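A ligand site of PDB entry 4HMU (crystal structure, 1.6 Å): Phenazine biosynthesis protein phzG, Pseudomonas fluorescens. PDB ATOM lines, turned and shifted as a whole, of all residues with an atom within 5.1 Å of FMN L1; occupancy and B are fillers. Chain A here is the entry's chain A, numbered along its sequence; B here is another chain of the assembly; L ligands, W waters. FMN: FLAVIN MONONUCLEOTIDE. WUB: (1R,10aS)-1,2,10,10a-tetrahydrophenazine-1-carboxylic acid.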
ATOM      1  N   GLU A  58     -10.131 -26.089 -22.950  1.00  0.00           N
ATOM      2  CA  GLU A  58      -9.552 -25.308 -24.056  1.00  0.00           C
ATOM      3  C   GLU A  58      -8.308 -25.945 -24.655  1.00  0.00           C
ATOM      4  O   GLU A  58      -7.206 -25.368 -24.661  1.00  0.00           O
ATOM      5  CB  GLU A  58      -9.292 -23.867 -23.629  1.00  0.00           C
ATOM      6  CG  GLU A  58     -10.555 -23.118 -23.248  1.00  0.00           C
ATOM      7  CD  GLU A  58     -10.288 -21.656 -22.959  1.00  0.00           C
ATOM      8  OE1 GLU A  58      -9.441 -21.036 -23.640  1.00  0.00           O
ATOM      9  OE2 GLU A  58     -10.938 -21.113 -22.029  1.00  0.00           O
ATOM     10  N   ALA A  61      -6.270 -23.942 -27.576  1.00  0.00           N
ATOM     11  CA  ALA A  61      -5.635 -22.659 -27.304  1.00  0.00           C
ATOM     12  C   ALA A  61      -4.130 -22.768 -27.559  1.00  0.00           C
ATOM     13  O   ALA A  61      -3.379 -23.333 -26.764  1.00  0.00           O
ATOM     14  CB  ALA A  61      -5.919 -22.215 -25.879  1.00  0.00           C
ATOM     15  N   THR A  75       4.566 -13.471 -29.206  1.00  0.00           N
ATOM     16  CA  THR A  75       3.651 -14.562 -28.902  1.00  0.00           C
ATOM     17  C   THR A  75       2.284 -14.031 -28.506  1.00  0.00           C
ATOM     18  O   THR A  75       2.125 -12.868 -28.117  1.00  0.00           O
ATOM     19  CB  THR A  75       4.153 -15.430 -27.732  1.00  0.00           C
ATOM     20  OG1 THR A  75       4.375 -14.613 -26.577  1.00  0.00           O
ATOM     21  CG2 THR A  75       5.422 -16.157 -28.113  1.00  0.00           C
ATOM     22  N   ARG A  76       1.290 -14.907 -28.629  1.00  0.00           N
ATOM     23  CA  ARG A  76      -0.080 -14.661 -28.168  1.00  0.00           C
ATOM     24  C   ARG A  76      -0.839 -15.969 -28.333  1.00  0.00           C
ATOM     25  O   ARG A  76      -0.393 -16.857 -29.050  1.00  0.00           O
ATOM     26  CB  ARG A  76      -0.757 -13.576 -28.992  1.00  0.00           C
ATOM     27  CG  ARG A  76      -1.197 -14.023 -30.381  1.00  0.00           C
ATOM     28  CD  ARG A  76      -0.007 -14.309 -31.272  1.00  0.00           C
ATOM     29  NE  ARG A  76       0.714 -13.082 -31.592  1.00  0.00           N
ATOM     30  CZ  ARG A  76       1.895 -13.025 -32.196  1.00  0.00           C
ATOM     31  NH1 ARG A  76       2.438 -11.847 -32.467  1.00  0.00           N
ATOM     32  NH2 ARG A  76       2.528 -14.142 -32.542  1.00  0.00           N
ATOM     33  N   ILE A  77      -1.994 -16.069 -27.684  1.00  0.00           N
ATOM     34  CA  ILE A  77      -2.876 -17.212 -27.906  1.00  0.00           C
ATOM     35  C   ILE A  77      -3.769 -16.992 -29.135  1.00  0.00           C
ATOM     36  O   ILE A  77      -4.331 -15.920 -29.323  1.00  0.00           O
ATOM     37  CB  ILE A  77      -3.804 -17.468 -26.688  1.00  0.00           C
ATOM     38  CG1 ILE A  77      -3.008 -17.672 -25.397  1.00  0.00           C
ATOM     39  CG2 ILE A  77      -4.720 -18.666 -26.948  1.00  0.00           C
ATOM     40  CD1 ILE A  77      -2.109 -18.902 -25.408  1.00  0.00           C
ATOM     41  N   VAL A  78      -3.875 -18.019 -29.978  1.00  0.00           N
ATOM     42  CA  VAL A  78      -4.926 -18.093 -30.994  1.00  0.00           C
ATOM     43  C   VAL A  78      -5.587 -19.458 -30.876  1.00  0.00           C
ATOM     44  O   VAL A  78      -5.013 -20.374 -30.283  1.00  0.00           O
ATOM     45  CB  VAL A  78      -4.408 -17.899 -32.444  1.00  0.00           C
ATOM     46  CG1 VAL A  78      -3.754 -16.523 -32.587  1.00  0.00           C
ATOM     47  CG2 VAL A  78      -3.440 -19.034 -32.885  1.00  0.00           C
ATOM     48  N   VAL A  79      -6.799 -19.576 -31.403  1.00  0.00           N
ATOM     49  CA  VAL A  79      -7.497 -20.854 -31.379  1.00  0.00           C
ATOM     50  C   VAL A  79      -7.347 -21.569 -32.733  1.00  0.00           C
ATOM     51  O   VAL A  79      -7.561 -20.985 -33.789  1.00  0.00           O
ATOM     52  CB  VAL A  79      -8.990 -20.702 -30.932  1.00  0.00           C
ATOM     53  CG1 VAL A  79      -9.810 -19.898 -31.920  1.00  0.00           C
ATOM     54  CG2 VAL A  79      -9.626 -22.074 -30.688  1.00  0.00           C
ATOM     55  N   SER A  91      -7.685 -18.165 -37.634  1.00  0.00           N
ATOM     56  CA  SER A  91      -8.049 -16.895 -38.237  1.00  0.00           C
ATOM     57  C   SER A  91      -7.491 -15.738 -37.418  1.00  0.00           C
ATOM     58  O   SER A  91      -7.258 -15.866 -36.233  1.00  0.00           O
ATOM     59  CB  SER A  91      -9.561 -16.769 -38.367  1.00  0.00           C
ATOM     60  OG  SER A  91     -10.179 -16.596 -37.099  1.00  0.00           O
ATOM     61  N   THR A  92      -7.290 -14.597 -38.059  1.00  0.00           N
ATOM     62  CA  THR A  92      -6.811 -13.414 -37.365  1.00  0.00           C
ATOM     63  C   THR A  92      -7.009 -12.200 -38.246  1.00  0.00           C
ATOM     64  O   THR A  92      -7.679 -12.282 -39.278  1.00  0.00           O
ATOM     65  CB  THR A  92      -5.318 -13.569 -36.952  1.00  0.00           C
ATOM     66  OG1 THR A  92      -4.967 -12.540 -36.014  1.00  0.00           O
ATOM     67  CG2 THR A  92      -4.392 -13.511 -38.154  1.00  0.00           C
ATOM     68  N   HIS A  93      -6.472 -11.059 -37.847  1.00  0.00           N
ATOM     69  CA  HIS A  93      -6.473  -9.880 -38.699  1.00  0.00           C
ATOM     70  C   HIS A  93      -5.108  -9.666 -39.337  1.00  0.00           C
ATOM     71  O   HIS A  93      -4.072  -9.758 -38.674  1.00  0.00           O
ATOM     72  CB  HIS A  93      -6.914  -8.656 -37.913  1.00  0.00           C
ATOM     73  CG  HIS A  93      -8.324  -8.752 -37.417  1.00  0.00           C
ATOM     74  ND1 HIS A  93      -9.387  -8.192 -38.086  1.00  0.00           N
ATOM     75  CD2 HIS A  93      -8.845  -9.390 -36.344  1.00  0.00           C
ATOM     76  CE1 HIS A  93     -10.508  -8.462 -37.443  1.00  0.00           C
ATOM     77  NE2 HIS A  93     -10.209  -9.182 -36.378  1.00  0.00           N
ATOM     78  N   SER A  96      -2.702  -7.131 -37.802  1.00  0.00           N
ATOM     79  CA  SER A  96      -2.224  -7.353 -36.429  1.00  0.00           C
ATOM     80  C   SER A  96      -0.711  -7.543 -36.441  1.00  0.00           C
ATOM     81  O   SER A  96      -0.093  -7.611 -37.517  1.00  0.00           O
ATOM     82  CB  SER A  96      -2.901  -8.568 -35.820  1.00  0.00           C
ATOM     83  OG  SER A  96      -2.537  -9.740 -36.551  1.00  0.00           O
ATOM     84  N   GLN A  97      -0.103  -7.635 -35.268  1.00  0.00           N
ATOM     85  CA  GLN A  97       1.331  -7.880 -35.207  1.00  0.00           C
ATOM     86  C   GLN A  97       1.674  -9.227 -35.826  1.00  0.00           C
ATOM     87  O   GLN A  97       2.626  -9.343 -36.591  1.00  0.00           O
ATOM     88  CB  GLN A  97       1.881  -7.779 -33.783  1.00  0.00           C
ATOM     89  CG  GLN A  97       3.374  -8.061 -33.710  1.00  0.00           C
ATOM     90  CD  GLN A  97       3.992  -7.751 -32.365  1.00  0.00           C
ATOM     91  OE1 GLN A  97       3.320  -7.350 -31.421  1.00  0.00           O
ATOM     92  NE2 GLN A  97       5.296  -7.935 -32.269  1.00  0.00           N
ATOM     93  N   LYS A  98       0.920 -10.275 -35.479  1.00  0.00           N
ATOM     94  CA  LYS A  98       1.223 -11.593 -36.008  1.00  0.00           C
ATOM     95  C   LYS A  98       1.010 -11.599 -37.525  1.00  0.00           C
ATOM     96  O   LYS A  98       1.755 -12.249 -38.243  1.00  0.00           O
ATOM     97  CB  LYS A  98       0.399 -12.690 -35.332  1.00  0.00           C
ATOM     98  CG  LYS A  98      -0.980 -12.932 -35.927  1.00  0.00           C
ATOM     99  CD  LYS A  98      -1.886 -13.773 -35.014  1.00  0.00           C
ATOM    100  CE  LYS A  98      -2.389 -12.987 -33.810  1.00  0.00           C
ATOM    101  NZ  LYS A  98      -2.974 -11.668 -34.218  1.00  0.00           N
ATOM    102  N   GLY A  99       0.027 -10.867 -38.011  1.00  0.00           N
ATOM    103  CA  GLY A  99      -0.268 -10.824 -39.433  1.00  0.00           C
ATOM    104  C   GLY A  99       0.856 -10.163 -40.214  1.00  0.00           C
ATOM    105  O   GLY A  99       1.298 -10.657 -41.251  1.00  0.00           O
ATOM    106  N   GLN A 155      -7.175  -4.594 -35.252  1.00  0.00           N
ATOM    107  CA  GLN A 155      -6.474  -5.359 -34.234  1.00  0.00           C
ATOM    108  C   GLN A 155      -5.013  -4.942 -34.060  1.00  0.00           C
ATOM    109  O   GLN A 155      -4.263  -4.905 -35.024  1.00  0.00           O
ATOM    110  CB  GLN A 155      -6.553  -6.845 -34.584  1.00  0.00           C
ATOM    111  CG  GLN A 155      -6.100  -7.761 -33.502  1.00  0.00           C
ATOM    112  CD  GLN A 155      -6.265  -9.212 -33.874  1.00  0.00           C
ATOM    113  OE1 GLN A 155      -5.639  -9.693 -34.816  1.00  0.00           O
ATOM    114  NE2 GLN A 155      -7.113  -9.933 -33.141  1.00  0.00           N
ATOM    115  N   SER A 156      -4.655  -4.608 -32.818  1.00  0.00           N
ATOM    116  CA  SER A 156      -3.278  -4.314 -32.408  1.00  0.00           C
ATOM    117  C   SER A 156      -2.808  -2.900 -32.702  1.00  0.00           C
ATOM    118  O   SER A 156      -1.710  -2.508 -32.291  1.00  0.00           O
ATOM    119  CB  SER A 156      -2.304  -5.349 -32.983  1.00  0.00           C
ATOM    120  OG  SER A 156      -2.773  -6.662 -32.675  1.00  0.00           O
ATOM    121  N   SER B  21     -14.469 -19.874 -27.814  1.00  0.00           N
ATOM    122  CA  SER B  21     -13.753 -20.910 -27.076  1.00  0.00           C
ATOM    123  C   SER B  21     -13.461 -20.550 -25.625  1.00  0.00           C
ATOM    124  O   SER B  21     -13.073 -21.439 -24.865  1.00  0.00           O
ATOM    125  CB  SER B  21     -12.449 -21.276 -27.772  1.00  0.00           C
ATOM    126  OG  SER B  21     -11.493 -20.220 -27.678  1.00  0.00           O
ATOM    127  N   LEU B  22     -13.609 -19.274 -25.251  1.00  0.00           N
ATOM    128  CA  LEU B  22     -13.286 -18.844 -23.891  1.00  0.00           C
ATOM    129  C   LEU B  22     -14.210 -19.506 -22.882  1.00  0.00           C
ATOM    130  O   LEU B  22     -15.423 -19.524 -23.056  1.00  0.00           O
ATOM    131  CB  LEU B  22     -13.387 -17.321 -23.702  1.00  0.00           C
ATOM    132  CG  LEU B  22     -12.430 -16.410 -24.455  1.00  0.00           C
ATOM    133  CD1 LEU B  22     -12.730 -14.953 -24.107  1.00  0.00           C
ATOM    134  CD2 LEU B  22     -10.995 -16.725 -24.113  1.00  0.00           C
ATOM    135  N   TYR B 113      -1.246 -17.797 -20.095  1.00  0.00           N
ATOM    136  CA  TYR B 113      -2.675 -17.737 -20.362  1.00  0.00           C
ATOM    137  C   TYR B 113      -3.389 -18.498 -19.261  1.00  0.00           C
ATOM    138  O   TYR B 113      -3.078 -19.679 -19.013  1.00  0.00           O
ATOM    139  CB  TYR B 113      -3.024 -18.313 -21.740  1.00  0.00           C
ATOM    140  CG  TYR B 113      -4.527 -18.466 -21.951  1.00  0.00           C
ATOM    141  CD1 TYR B 113      -5.408 -17.420 -21.674  1.00  0.00           C
ATOM    142  CD2 TYR B 113      -5.076 -19.663 -22.413  1.00  0.00           C
ATOM    143  CE1 TYR B 113      -6.777 -17.574 -21.838  1.00  0.00           C
ATOM    144  CE2 TYR B 113      -6.441 -19.818 -22.586  1.00  0.00           C
ATOM    145  CZ  TYR B 113      -7.289 -18.763 -22.299  1.00  0.00           C
ATOM    146  OH  TYR B 113      -8.656 -18.904 -22.474  1.00  0.00           O
ATOM    147  N   GLN B 120      -4.373 -13.028 -20.343  1.00  0.00           N
ATOM    148  CA  GLN B 120      -3.074 -13.342 -20.950  1.00  0.00           C
ATOM    149  C   GLN B 120      -2.079 -12.312 -20.500  1.00  0.00           C
ATOM    150  O   GLN B 120      -2.415 -11.135 -20.364  1.00  0.00           O
ATOM    151  CB  GLN B 120      -3.037 -13.235 -22.485  1.00  0.00           C
ATOM    152  CG  GLN B 120      -3.849 -14.103 -23.321  1.00  0.00           C
ATOM    153  CD  GLN B 120      -3.490 -13.828 -24.790  1.00  0.00           C
ATOM    154  OE1 GLN B 120      -2.568 -14.431 -25.355  1.00  0.00           O
ATOM    155  NE2 GLN B 120      -4.184 -12.868 -25.376  1.00  0.00           N
ATOM    156  N   GLU B 196       2.429  -7.045 -22.519  1.00  0.00           N
ATOM    157  CA  GLU B 196       1.003  -6.783 -22.695  1.00  0.00           C
ATOM    158  C   GLU B 196       0.199  -7.563 -21.656  1.00  0.00           C
ATOM    159  O   GLU B 196       0.470  -8.738 -21.401  1.00  0.00           O
ATOM    160  CB  GLU B 196       0.501  -7.150 -24.102  1.00  0.00           C
ATOM    161  CG  GLU B 196      -1.001  -6.897 -24.250  1.00  0.00           C
ATOM    162  CD  GLU B 196      -1.579  -7.305 -25.595  1.00  0.00           C
ATOM    163  OE1 GLU B 196      -0.847  -7.204 -26.613  1.00  0.00           O
ATOM    164  OE2 GLU B 196      -2.768  -7.726 -25.621  1.00  0.00           O
ATOM    165  N   TRP B 198      -3.679  -8.695 -21.111  1.00  0.00           N
ATOM    166  CA  TRP B 198      -4.903  -8.902 -21.868  1.00  0.00           C
ATOM    167  C   TRP B 198      -5.992  -9.448 -20.957  1.00  0.00           C
ATOM    168  O   TRP B 198      -5.779 -10.430 -20.250  1.00  0.00           O
ATOM    169  CB  TRP B 198      -4.633  -9.906 -22.986  1.00  0.00           C
ATOM    170  CG  TRP B 198      -5.724 -10.140 -24.013  1.00  0.00           C
ATOM    171  CD1 TRP B 198      -5.731  -9.668 -25.297  1.00  0.00           C
ATOM    172  CD2 TRP B 198      -6.916 -10.944 -23.881  1.00  0.00           C
ATOM    173  NE1 TRP B 198      -6.840 -10.107 -25.952  1.00  0.00           N
ATOM    174  CE2 TRP B 198      -7.593 -10.875 -25.109  1.00  0.00           C
ATOM    175  CE3 TRP B 198      -7.477 -11.687 -22.835  1.00  0.00           C
ATOM    176  CZ2 TRP B 198      -8.803 -11.539 -25.335  1.00  0.00           C
ATOM    177  CZ3 TRP B 198      -8.681 -12.343 -23.060  1.00  0.00           C
ATOM    178  CH2 TRP B 198      -9.333 -12.268 -24.300  1.00  0.00           C
ATOM    179  N   ARG B 208      -6.558  -4.524 -23.633  1.00  0.00           N
ATOM    180  CA  ARG B 208      -5.166  -4.775 -23.958  1.00  0.00           C
ATOM    181  C   ARG B 208      -4.340  -3.577 -23.517  1.00  0.00           C
ATOM    182  O   ARG B 208      -4.477  -2.472 -24.038  1.00  0.00           O
ATOM    183  CB  ARG B 208      -4.982  -4.991 -25.458  1.00  0.00           C
ATOM    184  CG  ARG B 208      -5.844  -6.105 -26.036  1.00  0.00           C
ATOM    185  CD  ARG B 208      -5.569  -6.293 -27.527  1.00  0.00           C
ATOM    186  NE  ARG B 208      -4.186  -6.699 -27.758  1.00  0.00           N
ATOM    187  CZ  ARG B 208      -3.620  -6.832 -28.952  1.00  0.00           C
ATOM    188  NH1 ARG B 208      -4.319  -6.588 -30.053  1.00  0.00           N
ATOM    189  NH2 ARG B 208      -2.357  -7.217 -29.056  1.00  0.00           N
ATOM    190  N   PRO B 225      -8.627  -4.554 -29.846  1.00  0.00           N
ATOM    191  CA  PRO B 225      -8.755  -6.003 -29.663  1.00  0.00           C
ATOM    192  C   PRO B 225      -8.709  -6.802 -30.950  1.00  0.00           C
ATOM    193  O   PRO B 225      -8.298  -7.971 -30.913  1.00  0.00           O
ATOM    194  CB  PRO B 225     -10.130  -6.163 -28.990  1.00  0.00           C
ATOM    195  CG  PRO B 225     -10.876  -4.932 -29.340  1.00  0.00           C
ATOM    196  CD  PRO B 225      -9.855  -3.832 -29.471  1.00  0.00           C
ATOM    197  OXT PRO B 225      -9.078  -6.323 -32.031  1.00  0.00           O
HETATM  198  N1  FMN L   1      -6.789 -13.477 -31.790  1.00  0.00           N
HETATM  199  C2  FMN L   1      -6.941 -13.808 -33.110  1.00  0.00           C
HETATM  200  O2  FMN L   1      -6.675 -12.986 -33.989  1.00  0.00           O
HETATM  201  N3  FMN L   1      -7.364 -15.065 -33.460  1.00  0.00           N
HETATM  202  C4  FMN L   1      -7.679 -16.004 -32.514  1.00  0.00           C
HETATM  203  O4  FMN L   1      -8.048 -17.118 -32.889  1.00  0.00           O
HETATM  204  C4A FMN L   1      -7.547 -15.673 -31.180  1.00  0.00           C
HETATM  205  N5  FMN L   1      -7.860 -16.585 -30.182  1.00  0.00           N
HETATM  206  C5A FMN L   1      -7.685 -16.247 -28.866  1.00  0.00           C
HETATM  207  C6  FMN L   1      -7.976 -17.187 -27.880  1.00  0.00           C
HETATM  208  C7  FMN L   1      -7.830 -16.869 -26.539  1.00  0.00           C
HETATM  209  C7M FMN L   1      -8.144 -17.905 -25.500  1.00  0.00           C
HETATM  210  C8  FMN L   1      -7.387 -15.603 -26.183  1.00  0.00           C
HETATM  211  C8M FMN L   1      -7.195 -15.237 -24.746  1.00  0.00           C
HETATM  212  C9  FMN L   1      -7.092 -14.668 -27.157  1.00  0.00           C
HETATM  213  C9A FMN L   1      -7.249 -14.974 -28.513  1.00  0.00           C
HETATM  214  N10 FMN L   1      -6.971 -14.049 -29.502  1.00  0.00           N
HETATM  215  C10 FMN L   1      -7.098 -14.399 -30.822  1.00  0.00           C
HETATM  216  C1' FMN L   1      -6.427 -12.683 -29.204  1.00  0.00           C
HETATM  217  C2' FMN L   1      -4.903 -12.807 -29.335  1.00  0.00           C
HETATM  218  O2' FMN L   1      -4.350 -13.462 -28.197  1.00  0.00           O
HETATM  219  C3' FMN L   1      -4.215 -11.439 -29.507  1.00  0.00           C
HETATM  220  O3' FMN L   1      -4.624 -10.538 -28.482  1.00  0.00           O
HETATM  221  C4' FMN L   1      -4.546 -10.807 -30.853  1.00  0.00           C
HETATM  222  O4' FMN L   1      -4.685 -11.801 -31.848  1.00  0.00           O
HETATM  223  C5' FMN L   1      -3.477  -9.787 -31.236  1.00  0.00           C
HETATM  224  O5' FMN L   1      -2.213 -10.422 -31.276  1.00  0.00           O
HETATM  225  P   FMN L   1      -0.955  -9.675 -31.922  1.00  0.00           P
HETATM  226  O1P FMN L   1      -1.013  -9.917 -33.408  1.00  0.00           O
HETATM  227  O2P FMN L   1      -1.024  -8.211 -31.569  1.00  0.00           O
HETATM  228  O3P FMN L   1       0.269 -10.316 -31.307  1.00  0.00           O
HETATM  229  O01 WUB L   2     -12.431 -18.458 -29.179  1.00  0.00           O
HETATM  230  C02 WUB L   2     -12.587 -17.315 -29.742  1.00  0.00           C
HETATM  231  O03 WUB L   2     -13.469 -16.708 -30.469  1.00  0.00           O
HETATM  232  C04 WUB L   2     -11.434 -16.402 -29.482  1.00  0.00           C
HETATM  233  C05 WUB L   2     -11.493 -15.866 -28.061  1.00  0.00           C
HETATM  234  C06 WUB L   2     -10.894 -14.524 -27.742  1.00  0.00           C
HETATM  235  C07 WUB L   2     -10.503 -13.655 -28.719  1.00  0.00           C
HETATM  236  C08 WUB L   2     -10.682 -14.047 -30.139  1.00  0.00           C
HETATM  237  N09 WUB L   2     -10.203 -13.242 -31.091  1.00  0.00           N
HETATM  238  C10 WUB L   2     -10.348 -13.583 -32.451  1.00  0.00           C
HETATM  239  C11 WUB L   2     -10.033 -12.658 -33.459  1.00  0.00           C
HETATM  240  C12 WUB L   2     -10.143 -13.017 -34.805  1.00  0.00           C
HETATM  241  C13 WUB L   2     -10.562 -14.294 -35.141  1.00  0.00           C
HETATM  242  C14 WUB L   2     -10.862 -15.200 -34.161  1.00  0.00           C
HETATM  243  C15 WUB L   2     -10.742 -14.829 -32.781  1.00  0.00           C
HETATM  244  N16 WUB L   2     -11.048 -15.784 -31.788  1.00  0.00           N
HETATM  245  C17 WUB L   2     -11.478 -15.285 -30.503  1.00  0.00           C
HETATM  246  O   HOH W   1      -2.458 -10.196 -27.028  1.00  0.00           O
HETATM  247  O   HOH W   2      -8.632 -18.822 -34.988  1.00  0.00           O
HETATM  248  O   HOH W   3      -7.286  -9.293 -28.711  1.00  0.00           O
HETATM  249  O   HOH W   4       0.125 -10.059 -28.607  1.00  0.00           O
HETATM  250  O   HOH W   5       0.908  -6.666 -30.529  1.00  0.00           O
HETATM  251  O   HOH W   6       2.435 -10.512 -29.129  1.00  0.00           O
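O2 of FMN L1 is in hydrogen-bond range of NE2 of Gln 155 (3.2 Å).
The backbone NH (N) of Val 79 lies within hydrogen-bond range of an oxygen (O4) of FMN L1, 3.1 Å away.
The backbone NH (N) of Lys 98 is in hydrogen-bond range of an oxygen (O1P) of FMN L1 (2.9 Å).
OG1 of Thr 92 sits at hydrogen-bond distance from O2 of FMN L1 (2.7 Å).
N3 of FMN L1 sits at hydrogen-bond distance from O of Ser 91, at 2.9 Å.
The guanidinium group (NH2) of Arg 208 of chain B lies within salt-bridge range of an oxygen (O2P) of FMN L1 (3.0 Å).
OG of Ser 96 sits close to O1P of FMN L1 (3.5 Å).
The side-chain hydroxyl (OG) of Ser 21 of chain B is in hydrogen-bond range of an oxygen (O01) of WUB L2.
O1P of FMN L1 sits at hydrogen-bond distance from N of Gln 97, 3.1 Å away.
The side-chain amide nitrogen (NE2) of Gln 120 of chain B lies within hydrogen-bond range of an oxygen (O2') of FMN L1.
NE1 of Trp 198 of chain B sits at hydrogen-bond distance from O3' of FMN L1, at 3.4 Å.
An oxygen (O2') of FMN L1 sits at hydrogen-bond distance from the backbone carbonyl oxygen (O) of Ile 77, at 2.7 Å.
An oxygen (O1P) of FMN L1 is in salt-bridge range of the side-chain amino group (NZ) of Lys 98 (2.8 Å).
O01 of WUB L2 is in hydrogen-bond range of N of Ser 21 of chain B (2.8 Å).
The side-chain hydroxyl (OG) of Ser 156 is in hydrogen-bond range of an oxygen (O2P) of FMN L1 (2.6 Å).
An oxygen (O3P) of FMN L1 is in salt-bridge range of the guanidinium group (NE) of Arg 76 (2.8 Å).
N16 of WUB L2 lies close to O4 of FMN L1, at 3.5 Å.
The chain-end carboxylate (O) of Pro 225 of chain B lies within hydrogen-bond range of the side-chain amide nitrogen (NE2) of Gln 155.
The side-chain amide oxygen (OE1) of Gln 120 of chain B is in hydrogen-bond range of the backbone NH (N) of Ile 77 (2.9 Å).
The side-chain hydroxyl of Thr 92 is in hydrogen-bond range of the side-chain amino group of Lys 98 (2.8 Å).
N of Gly 99 sits at hydrogen-bond distance from OG of Ser 96 (3.2 Å).
O of Gln 120 of chain B sits at hydrogen-bond distance from N of Trp 198 of chain B.
NH1 of Arg 208 of chain B lies within hydrogen-bond range of OG of Ser 156 (3.0 Å).
NE of Arg 208 of chain B lies within salt-bridge range of OE2 of Glu 196 of chain B, 2.8 Å away.
The side-chain amino group (NZ) of Lys 98 is in hydrogen-bond range of the side-chain hydroxyl (OG) of Ser 96, 3.1 Å away.
OE1 of Glu 58 touches C7M of FMN L1, at 3.9 Å.
Val 78 touches FMN L1.
Leu 22 of chain B touches FMN L1 (CD2 to C7M, 3.4 Å).
Tyr 113 of chain B touches FMN L1 (OH to C7M, 3.2 Å).
Of the 24 residues printed, 17 come within 4 Å of FMN L1.
Water W1 bridges O3' of FMN L1 and OE2 of Glu 196 of chain B.
Water W5 bridges OE1 of Gln 97 and O2P of FMN L1.
Water W4 bridges an oxygen (O3P) of FMN L1 (2.7 Å) and the backbone carbonyl oxygen of Thr 75 (3.5 Å).
Water W2 lies within hydrogen-bond range of the backbone carbonyl oxygen of Val 79, an oxygen (O4) of FMN L1 and the backbone NH of Ser 91.
Water W3 lies within hydrogen-bond range of the chain-end carboxylate (O) of Pro 225 of chain B (2.8 Å), the indole nitrogen (NE1) of Trp 198 of chain B (2.9 Å) and an oxygen (O3') of FMN L1 (2.9 Å).
Water W6 bridges O of Thr 75 and O3P of FMN L1.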
